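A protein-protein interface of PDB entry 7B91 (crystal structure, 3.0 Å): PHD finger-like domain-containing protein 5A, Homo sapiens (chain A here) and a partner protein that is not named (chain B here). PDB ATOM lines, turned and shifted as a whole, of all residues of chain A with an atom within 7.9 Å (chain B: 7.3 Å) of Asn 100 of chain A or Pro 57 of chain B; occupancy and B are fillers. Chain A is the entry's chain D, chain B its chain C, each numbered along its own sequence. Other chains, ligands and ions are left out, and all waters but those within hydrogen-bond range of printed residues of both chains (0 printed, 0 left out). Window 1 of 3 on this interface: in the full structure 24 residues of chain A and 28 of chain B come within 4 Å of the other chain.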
ATOM      1  N   ASP A  17      -8.827   4.419 -30.022  1.00  0.00           N
ATOM      2  CA  ASP A  17      -9.873   5.361 -29.635  1.00  0.00           C
ATOM      3  C   ASP A  17      -9.560   6.033 -28.297  1.00  0.00           C
ATOM      4  O   ASP A  17      -9.899   7.197 -28.083  1.00  0.00           O
ATOM      5  CB  ASP A  17     -11.234   4.655 -29.572  1.00  0.00           C
ATOM      6  CG  ASP A  17     -11.177   3.329 -28.828  1.00  0.00           C
ATOM      7  OD1 ASP A  17     -12.196   2.956 -28.205  1.00  0.00           O
ATOM      8  OD2 ASP A  17     -10.124   2.658 -28.870  1.00  0.00           O
ATOM      9  N   LEU A  18      -8.910   5.293 -27.399  1.00  0.00           N
ATOM     10  CA  LEU A  18      -8.512   5.800 -26.092  1.00  0.00           C
ATOM     11  C   LEU A  18      -6.993   5.798 -26.008  1.00  0.00           C
ATOM     12  O   LEU A  18      -6.354   4.793 -26.336  1.00  0.00           O
ATOM     13  CB  LEU A  18      -9.102   4.952 -24.962  1.00  0.00           C
ATOM     14  CG  LEU A  18     -10.600   4.643 -25.008  1.00  0.00           C
ATOM     15  CD1 LEU A  18     -11.055   4.030 -23.693  1.00  0.00           C
ATOM     16  CD2 LEU A  18     -11.404   5.891 -25.322  1.00  0.00           C
ATOM     17  N   ILE A  19      -6.413   6.916 -25.566  1.00  0.00           N
ATOM     18  CA  ILE A  19      -4.959   7.036 -25.520  1.00  0.00           C
ATOM     19  C   ILE A  19      -4.552   7.755 -24.241  1.00  0.00           C
ATOM     20  O   ILE A  19      -5.327   8.504 -23.648  1.00  0.00           O
ATOM     21  CB  ILE A  19      -4.399   7.764 -26.768  1.00  0.00           C
ATOM     22  CG1 ILE A  19      -2.877   7.593 -26.877  1.00  0.00           C
ATOM     23  CG2 ILE A  19      -4.754   9.239 -26.732  1.00  0.00           C
ATOM     24  CD1 ILE A  19      -2.384   6.152 -26.749  1.00  0.00           C
ATOM     25  N   PHE A  20      -3.319   7.507 -23.807  1.00  0.00           N
ATOM     26  CA  PHE A  20      -2.795   8.195 -22.637  1.00  0.00           C
ATOM     27  C   PHE A  20      -2.459   9.645 -22.968  1.00  0.00           C
ATOM     28  O   PHE A  20      -2.008   9.961 -24.073  1.00  0.00           O
ATOM     29  CB  PHE A  20      -1.555   7.477 -22.105  1.00  0.00           C
ATOM     30  CG  PHE A  20      -1.832   6.105 -21.563  1.00  0.00           C
ATOM     31  CD1 PHE A  20      -2.752   5.923 -20.544  1.00  0.00           C
ATOM     32  CD2 PHE A  20      -1.164   4.999 -22.062  1.00  0.00           C
ATOM     33  CE1 PHE A  20      -3.009   4.664 -20.038  1.00  0.00           C
ATOM     34  CE2 PHE A  20      -1.414   3.736 -21.560  1.00  0.00           C
ATOM     35  CZ  PHE A  20      -2.339   3.568 -20.546  1.00  0.00           C
ATOM     36  N   LYS A  97      -3.272   9.773 -17.687  1.00  0.00           N
ATOM     37  CA  LYS A  97      -4.708   9.985 -17.807  1.00  0.00           C
ATOM     38  C   LYS A  97      -5.202   9.493 -19.162  1.00  0.00           C
ATOM     39  O   LYS A  97      -4.663   9.867 -20.207  1.00  0.00           O
ATOM     40  CB  LYS A  97      -5.048  11.466 -17.624  1.00  0.00           C
ATOM     41  CG  LYS A  97      -6.525  11.795 -17.807  1.00  0.00           C
ATOM     42  CD  LYS A  97      -7.262  11.866 -16.477  1.00  0.00           C
ATOM     43  CE  LYS A  97      -8.741  12.165 -16.678  1.00  0.00           C
ATOM     44  NZ  LYS A  97      -9.421  12.506 -15.397  1.00  0.00           N
ATOM     45  N   ILE A  98      -6.222   8.644 -19.142  1.00  0.00           N
ATOM     46  CA  ILE A  98      -6.802   8.138 -20.379  1.00  0.00           C
ATOM     47  C   ILE A  98      -7.749   9.186 -20.945  1.00  0.00           C
ATOM     48  O   ILE A  98      -8.651   9.666 -20.250  1.00  0.00           O
ATOM     49  CB  ILE A  98      -7.526   6.806 -20.139  1.00  0.00           C
ATOM     50  CG1 ILE A  98      -6.559   5.775 -19.555  1.00  0.00           C
ATOM     51  CG2 ILE A  98      -8.139   6.296 -21.435  1.00  0.00           C
ATOM     52  CD1 ILE A  98      -7.240   4.629 -18.847  1.00  0.00           C
ATOM     53  N   VAL A  99      -7.541   9.554 -22.207  1.00  0.00           N
ATOM     54  CA  VAL A  99      -8.378  10.521 -22.899  1.00  0.00           C
ATOM     55  C   VAL A  99      -9.047   9.827 -24.076  1.00  0.00           C
ATOM     56  O   VAL A  99      -8.446   8.970 -24.741  1.00  0.00           O
ATOM     57  CB  VAL A  99      -7.576  11.756 -23.365  1.00  0.00           C
ATOM     58  CG1 VAL A  99      -6.942  12.462 -22.172  1.00  0.00           C
ATOM     59  CG2 VAL A  99      -6.517  11.374 -24.387  1.00  0.00           C
ATOM     60  N   ASN A 100     -10.308  10.188 -24.307  1.00  0.00           N
ATOM     61  CA  ASN A 100     -11.107   9.675 -25.411  1.00  0.00           C
ATOM     62  C   ASN A 100     -11.080  10.709 -26.529  1.00  0.00           C
ATOM     63  O   ASN A 100     -11.466  11.864 -26.319  1.00  0.00           O
ATOM     64  CB  ASN A 100     -12.541   9.398 -24.952  1.00  0.00           C
ATOM     65  CG  ASN A 100     -13.391   8.730 -26.024  1.00  0.00           C
ATOM     66  OD1 ASN A 100     -13.411   9.155 -27.179  1.00  0.00           O
ATOM     67  ND2 ASN A 100     -14.116   7.687 -25.635  1.00  0.00           N
ATOM     68  N   LEU A 101     -10.624  10.298 -27.708  1.00  0.00           N
ATOM     69  CA  LEU A 101     -10.481  11.204 -28.838  1.00  0.00           C
ATOM     70  C   LEU A 101     -11.736  11.279 -29.700  1.00  0.00           C
ATOM     71  O   LEU A 101     -11.694  11.863 -30.788  1.00  0.00           O
ATOM     72  CB  LEU A 101      -9.277  10.794 -29.689  1.00  0.00           C
ATOM     73  CG  LEU A 101      -7.913  10.867 -28.993  1.00  0.00           C
ATOM     74  CD1 LEU A 101      -6.785  10.956 -30.007  1.00  0.00           C
ATOM     75  CD2 LEU A 101      -7.854  12.048 -28.033  1.00  0.00           C
ATOM     76  N   GLY A 102     -12.846  10.708 -29.241  1.00  0.00           N
ATOM     77  CA  GLY A 102     -14.098  10.812 -29.961  1.00  0.00           C
ATOM     78  C   GLY A 102     -15.190  11.428 -29.113  1.00  0.00           C
ATOM     79  O   GLY A 102     -16.378  11.167 -29.327  1.00  0.00           O
ATOM     80  N   SER A 103     -14.796  12.250 -28.140  1.00  0.00           N
ATOM     81  CA  SER A 103     -15.735  12.865 -27.212  1.00  0.00           C
ATOM     82  C   SER A 103     -15.330  14.307 -26.953  1.00  0.00           C
ATOM     83  O   SER A 103     -14.177  14.577 -26.603  1.00  0.00           O
ATOM     84  CB  SER A 103     -15.790  12.094 -25.888  1.00  0.00           C
ATOM     85  OG  SER A 103     -16.270  10.776 -26.081  1.00  0.00           O
ATOM     86  N   SER A 104     -16.278  15.227 -27.121  1.00  0.00           N
ATOM     87  CA  SER A 104     -16.048  16.612 -26.747  1.00  0.00           C
ATOM     88  C   SER A 104     -16.002  16.740 -25.225  1.00  0.00           C
ATOM     89  O   SER A 104     -16.312  15.805 -24.481  1.00  0.00           O
ATOM     90  CB  SER A 104     -17.138  17.512 -27.328  1.00  0.00           C
ATOM     91  OG  SER A 104     -17.360  17.227 -28.698  1.00  0.00           O
ATOM     92  N   LYS A 105     -15.611  17.924 -24.755  1.00  0.00           N
ATOM     93  CA  LYS A 105     -15.497  18.156 -23.321  1.00  0.00           C
ATOM     94  C   LYS A 105     -16.841  18.424 -22.654  1.00  0.00           C
ATOM     95  O   LYS A 105     -16.868  18.753 -21.464  1.00  0.00           O
ATOM     96  CB  LYS A 105     -14.532  19.315 -23.047  1.00  0.00           C
ATOM     97  CG  LYS A 105     -13.100  19.011 -23.466  1.00  0.00           C
ATOM     98  CD  LYS A 105     -12.121  20.125 -23.121  1.00  0.00           C
ATOM     99  CE  LYS A 105     -11.609  20.001 -21.695  1.00  0.00           C
ATOM    100  NZ  LYS A 105     -12.321  20.894 -20.744  1.00  0.00           N
ATOM    101  N   ASP A 107     -19.594  16.086 -23.408  1.00  0.00           N
ATOM    102  CA  ASP A 107     -20.314  14.817 -23.442  1.00  0.00           C
ATOM    103  C   ASP A 107     -20.269  14.116 -22.087  1.00  0.00           C
ATOM    104  O   ASP A 107     -21.227  13.453 -21.687  1.00  0.00           O
ATOM    105  CB  ASP A 107     -19.739  13.901 -24.527  1.00  0.00           C
ATOM    106  CG  ASP A 107     -19.767  14.539 -25.907  1.00  0.00           C
ATOM    107  OD1 ASP A 107     -20.221  15.698 -26.023  1.00  0.00           O
ATOM    108  OD2 ASP A 107     -19.332  13.882 -26.877  1.00  0.00           O
ATOM    109  N   GLY B  55     -16.329  19.716 -30.249  1.00  0.00           N
ATOM    110  CA  GLY B  55     -15.569  18.849 -31.125  1.00  0.00           C
ATOM    111  C   GLY B  55     -14.552  18.026 -30.366  1.00  0.00           C
ATOM    112  O   GLY B  55     -14.198  18.304 -29.222  1.00  0.00           O
ATOM    113  N   THR B  56     -14.069  16.981 -31.039  1.00  0.00           N
ATOM    114  CA  THR B  56     -13.080  16.085 -30.470  1.00  0.00           C
ATOM    115  C   THR B  56     -11.772  16.830 -30.201  1.00  0.00           C
ATOM    116  O   THR B  56     -11.543  17.917 -30.740  1.00  0.00           O
ATOM    117  CB  THR B  56     -12.846  14.908 -31.418  1.00  0.00           C
ATOM    118  OG1 THR B  56     -12.309  15.387 -32.657  1.00  0.00           O
ATOM    119  CG2 THR B  56     -14.153  14.174 -31.686  1.00  0.00           C
ATOM    120  N   PRO B  57     -10.912  16.276 -29.346  1.00  0.00           N
ATOM    121  CA  PRO B  57      -9.608  16.908 -29.075  1.00  0.00           C
ATOM    122  C   PRO B  57      -8.802  17.159 -30.340  1.00  0.00           C
ATOM    123  O   PRO B  57      -8.193  18.232 -30.466  1.00  0.00           O
ATOM    124  CB  PRO B  57      -8.912  15.897 -28.150  1.00  0.00           C
ATOM    125  CG  PRO B  57     -10.031  15.232 -27.437  1.00  0.00           C
ATOM    126  CD  PRO B  57     -11.185  15.168 -28.410  1.00  0.00           C
ATOM    127  N   PRO B  58      -8.748  16.220 -31.301  1.00  0.00           N
ATOM    128  CA  PRO B  58      -7.971  16.516 -32.521  1.00  0.00           C
ATOM    129  C   PRO B  58      -8.480  17.721 -33.295  1.00  0.00           C
ATOM    130  O   PRO B  58      -7.679  18.586 -33.681  1.00  0.00           O
ATOM    131  CB  PRO B  58      -8.085  15.217 -33.335  1.00  0.00           C
ATOM    132  CG  PRO B  58      -9.242  14.498 -32.764  1.00  0.00           C
ATOM    133  CD  PRO B  58      -9.208  14.819 -31.314  1.00  0.00           C
ATOM    134  N   MET B  59      -9.792  17.810 -33.538  1.00  0.00           N
ATOM    135  CA  MET B  59     -10.299  18.897 -34.370  1.00  0.00           C
ATOM    136  C   MET B  59     -10.208  20.238 -33.652  1.00  0.00           C
ATOM    137  O   MET B  59      -9.910  21.262 -34.279  1.00  0.00           O
ATOM    138  CB  MET B  59     -11.734  18.610 -34.821  1.00  0.00           C
ATOM    139  CG  MET B  59     -12.746  18.390 -33.713  1.00  0.00           C
ATOM    140  SD  MET B  59     -14.397  18.045 -34.371  1.00  0.00           S
ATOM    141  CE  MET B  59     -14.050  16.672 -35.468  1.00  0.00           C
ATOM    142  N   ARG B  60     -10.429  20.260 -32.334  1.00  0.00           N
ATOM    143  CA  ARG B  60     -10.275  21.525 -31.622  1.00  0.00           C
ATOM    144  C   ARG B  60      -8.808  21.921 -31.503  1.00  0.00           C
ATOM    145  O   ARG B  60      -8.494  23.113 -31.524  1.00  0.00           O
ATOM    146  CB  ARG B  60     -10.946  21.466 -30.247  1.00  0.00           C
ATOM    147  CG  ARG B  60     -10.304  20.554 -29.223  1.00  0.00           C
ATOM    148  CD  ARG B  60     -10.990  20.728 -27.872  1.00  0.00           C
ATOM    149  NE  ARG B  60     -11.433  19.458 -27.303  1.00  0.00           N
ATOM    150  CZ  ARG B  60     -10.879  18.878 -26.242  1.00  0.00           C
ATOM    151  NH1 ARG B  60      -9.858  19.454 -25.621  1.00  0.00           N
ATOM    152  NH2 ARG B  60     -11.350  17.720 -25.799  1.00  0.00           N
ATOM    153  N   LYS B  61      -7.897  20.947 -31.419  1.00  0.00           N
ATOM    154  CA  LYS B  61      -6.471  21.265 -31.466  1.00  0.00           C
ATOM    155  C   LYS B  61      -6.098  21.883 -32.809  1.00  0.00           C
ATOM    156  O   LYS B  61      -5.385  22.894 -32.870  1.00  0.00           O
ATOM    157  CB  LYS B  61      -5.649  20.004 -31.195  1.00  0.00           C
ATOM    158  CG  LYS B  61      -4.133  20.206 -31.183  1.00  0.00           C
ATOM    159  CD  LYS B  61      -3.506  19.917 -32.545  1.00  0.00           C
ATOM    160  CE  LYS B  61      -2.144  20.580 -32.688  1.00  0.00           C
ATOM    161  NZ  LYS B  61      -1.890  21.018 -34.089  1.00  0.00           N
ATOM    162  N   ALA B  62      -6.572  21.277 -33.901  1.00  0.00           N
ATOM    163  CA  ALA B  62      -6.304  21.822 -35.228  1.00  0.00           C
ATOM    164  C   ALA B  62      -6.879  23.224 -35.374  1.00  0.00           C
ATOM    165  O   ALA B  62      -6.224  24.120 -35.921  1.00  0.00           O
ATOM    166  CB  ALA B  62      -6.870  20.894 -36.302  1.00  0.00           C
ATOM    167  N   ALA B  63      -8.099  23.440 -34.875  1.00  0.00           N
ATOM    168  CA  ALA B  63      -8.722  24.754 -34.991  1.00  0.00           C
ATOM    169  C   ALA B  63      -8.003  25.789 -34.134  1.00  0.00           C
ATOM    170  O   ALA B  63      -7.877  26.952 -34.533  1.00  0.00           O
ATOM    171  CB  ALA B  63     -10.199  24.667 -34.613  1.00  0.00           C
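Asn 100 of chain A touches just one residue of chain B: Pro 57 (3.8 Å). Of the printed residues of chain B, Gly 102 of chain A touches Thr 56. Of chain A, only Asn 100 (3.8 Å), Leu 101 (3.9 Å) and Ser 103 (3.5 Å) come within 4 Å of Pro 57 of chain B. Printed residues of chain A within 4 Å of Arg 60 of chain B: Lys 105 (3.2 Å). The nearest residue of chain B that does not touch Asn 100 of chain A is Arg 60 of chain B (5.9 Å). The nearest printed residue of chain B that does not touch Gly 102 of chain A is Pro 57 of chain B (4.8 Å).
The side-chain hydroxyl (OG) of Ser 104 of chain A sits at hydrogen-bond distance from the backbone NH (N) of Gly 55 of chain B (3.1 Å).
N of Thr 56 of chain B lies close to SD of Met 59 of chain B. The side-chain amide oxygen of Asn 100 of chain A is in hydrogen-bond range of the backbone NH of Gly 102 of chain A, at 2.6 Å. The backbone NH (N) of Leu 101 of chain A sits at hydrogen-bond distance from the backbone carbonyl oxygen (O) of Asp 17 of chain A (3.2 Å). The side-chain amide oxygen (OD1) of Asn 100 of chain A is in hydrogen-bond range of the side-chain hydroxyl (OG) of Ser 103 of chain A (3.5 Å). The side-chain carboxylate (OD2) of Asp 107 of chain A sits at hydrogen-bond distance from the backbone NH (N) of Ser 104 of chain A, at 3.3 Å.
Hydrophobic or aromatic side chains of chain A that line the printed part of chain B: Leu 101. Of the 9 printed residues of chain B, 5 touch a printed residue of chain A. Hydrophobic or aromatic side chains of chain B that line the printed part of chain A: Pro 57 and Pro 58.
Among the printed residues, pairs that only touch across the chains: Asn 100 of chain A with Pro 57 of chain B (3.8 Å), Leu 101 of chain A with Thr 56 of chain B (3.3 Å), Leu 101 of chain A with Pro 57 of chain B (3.9 Å), Leu 101 of chain A with Pro 58 of chain B (3.9 Å), Gly 102 of chain A with Thr 56 of chain B (3.8 Å), Ser 103 of chain A with Pro 57 of chain B (3.5 Å) and Lys 105 of chain A with Arg 60 of chain B (3.2 Å).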
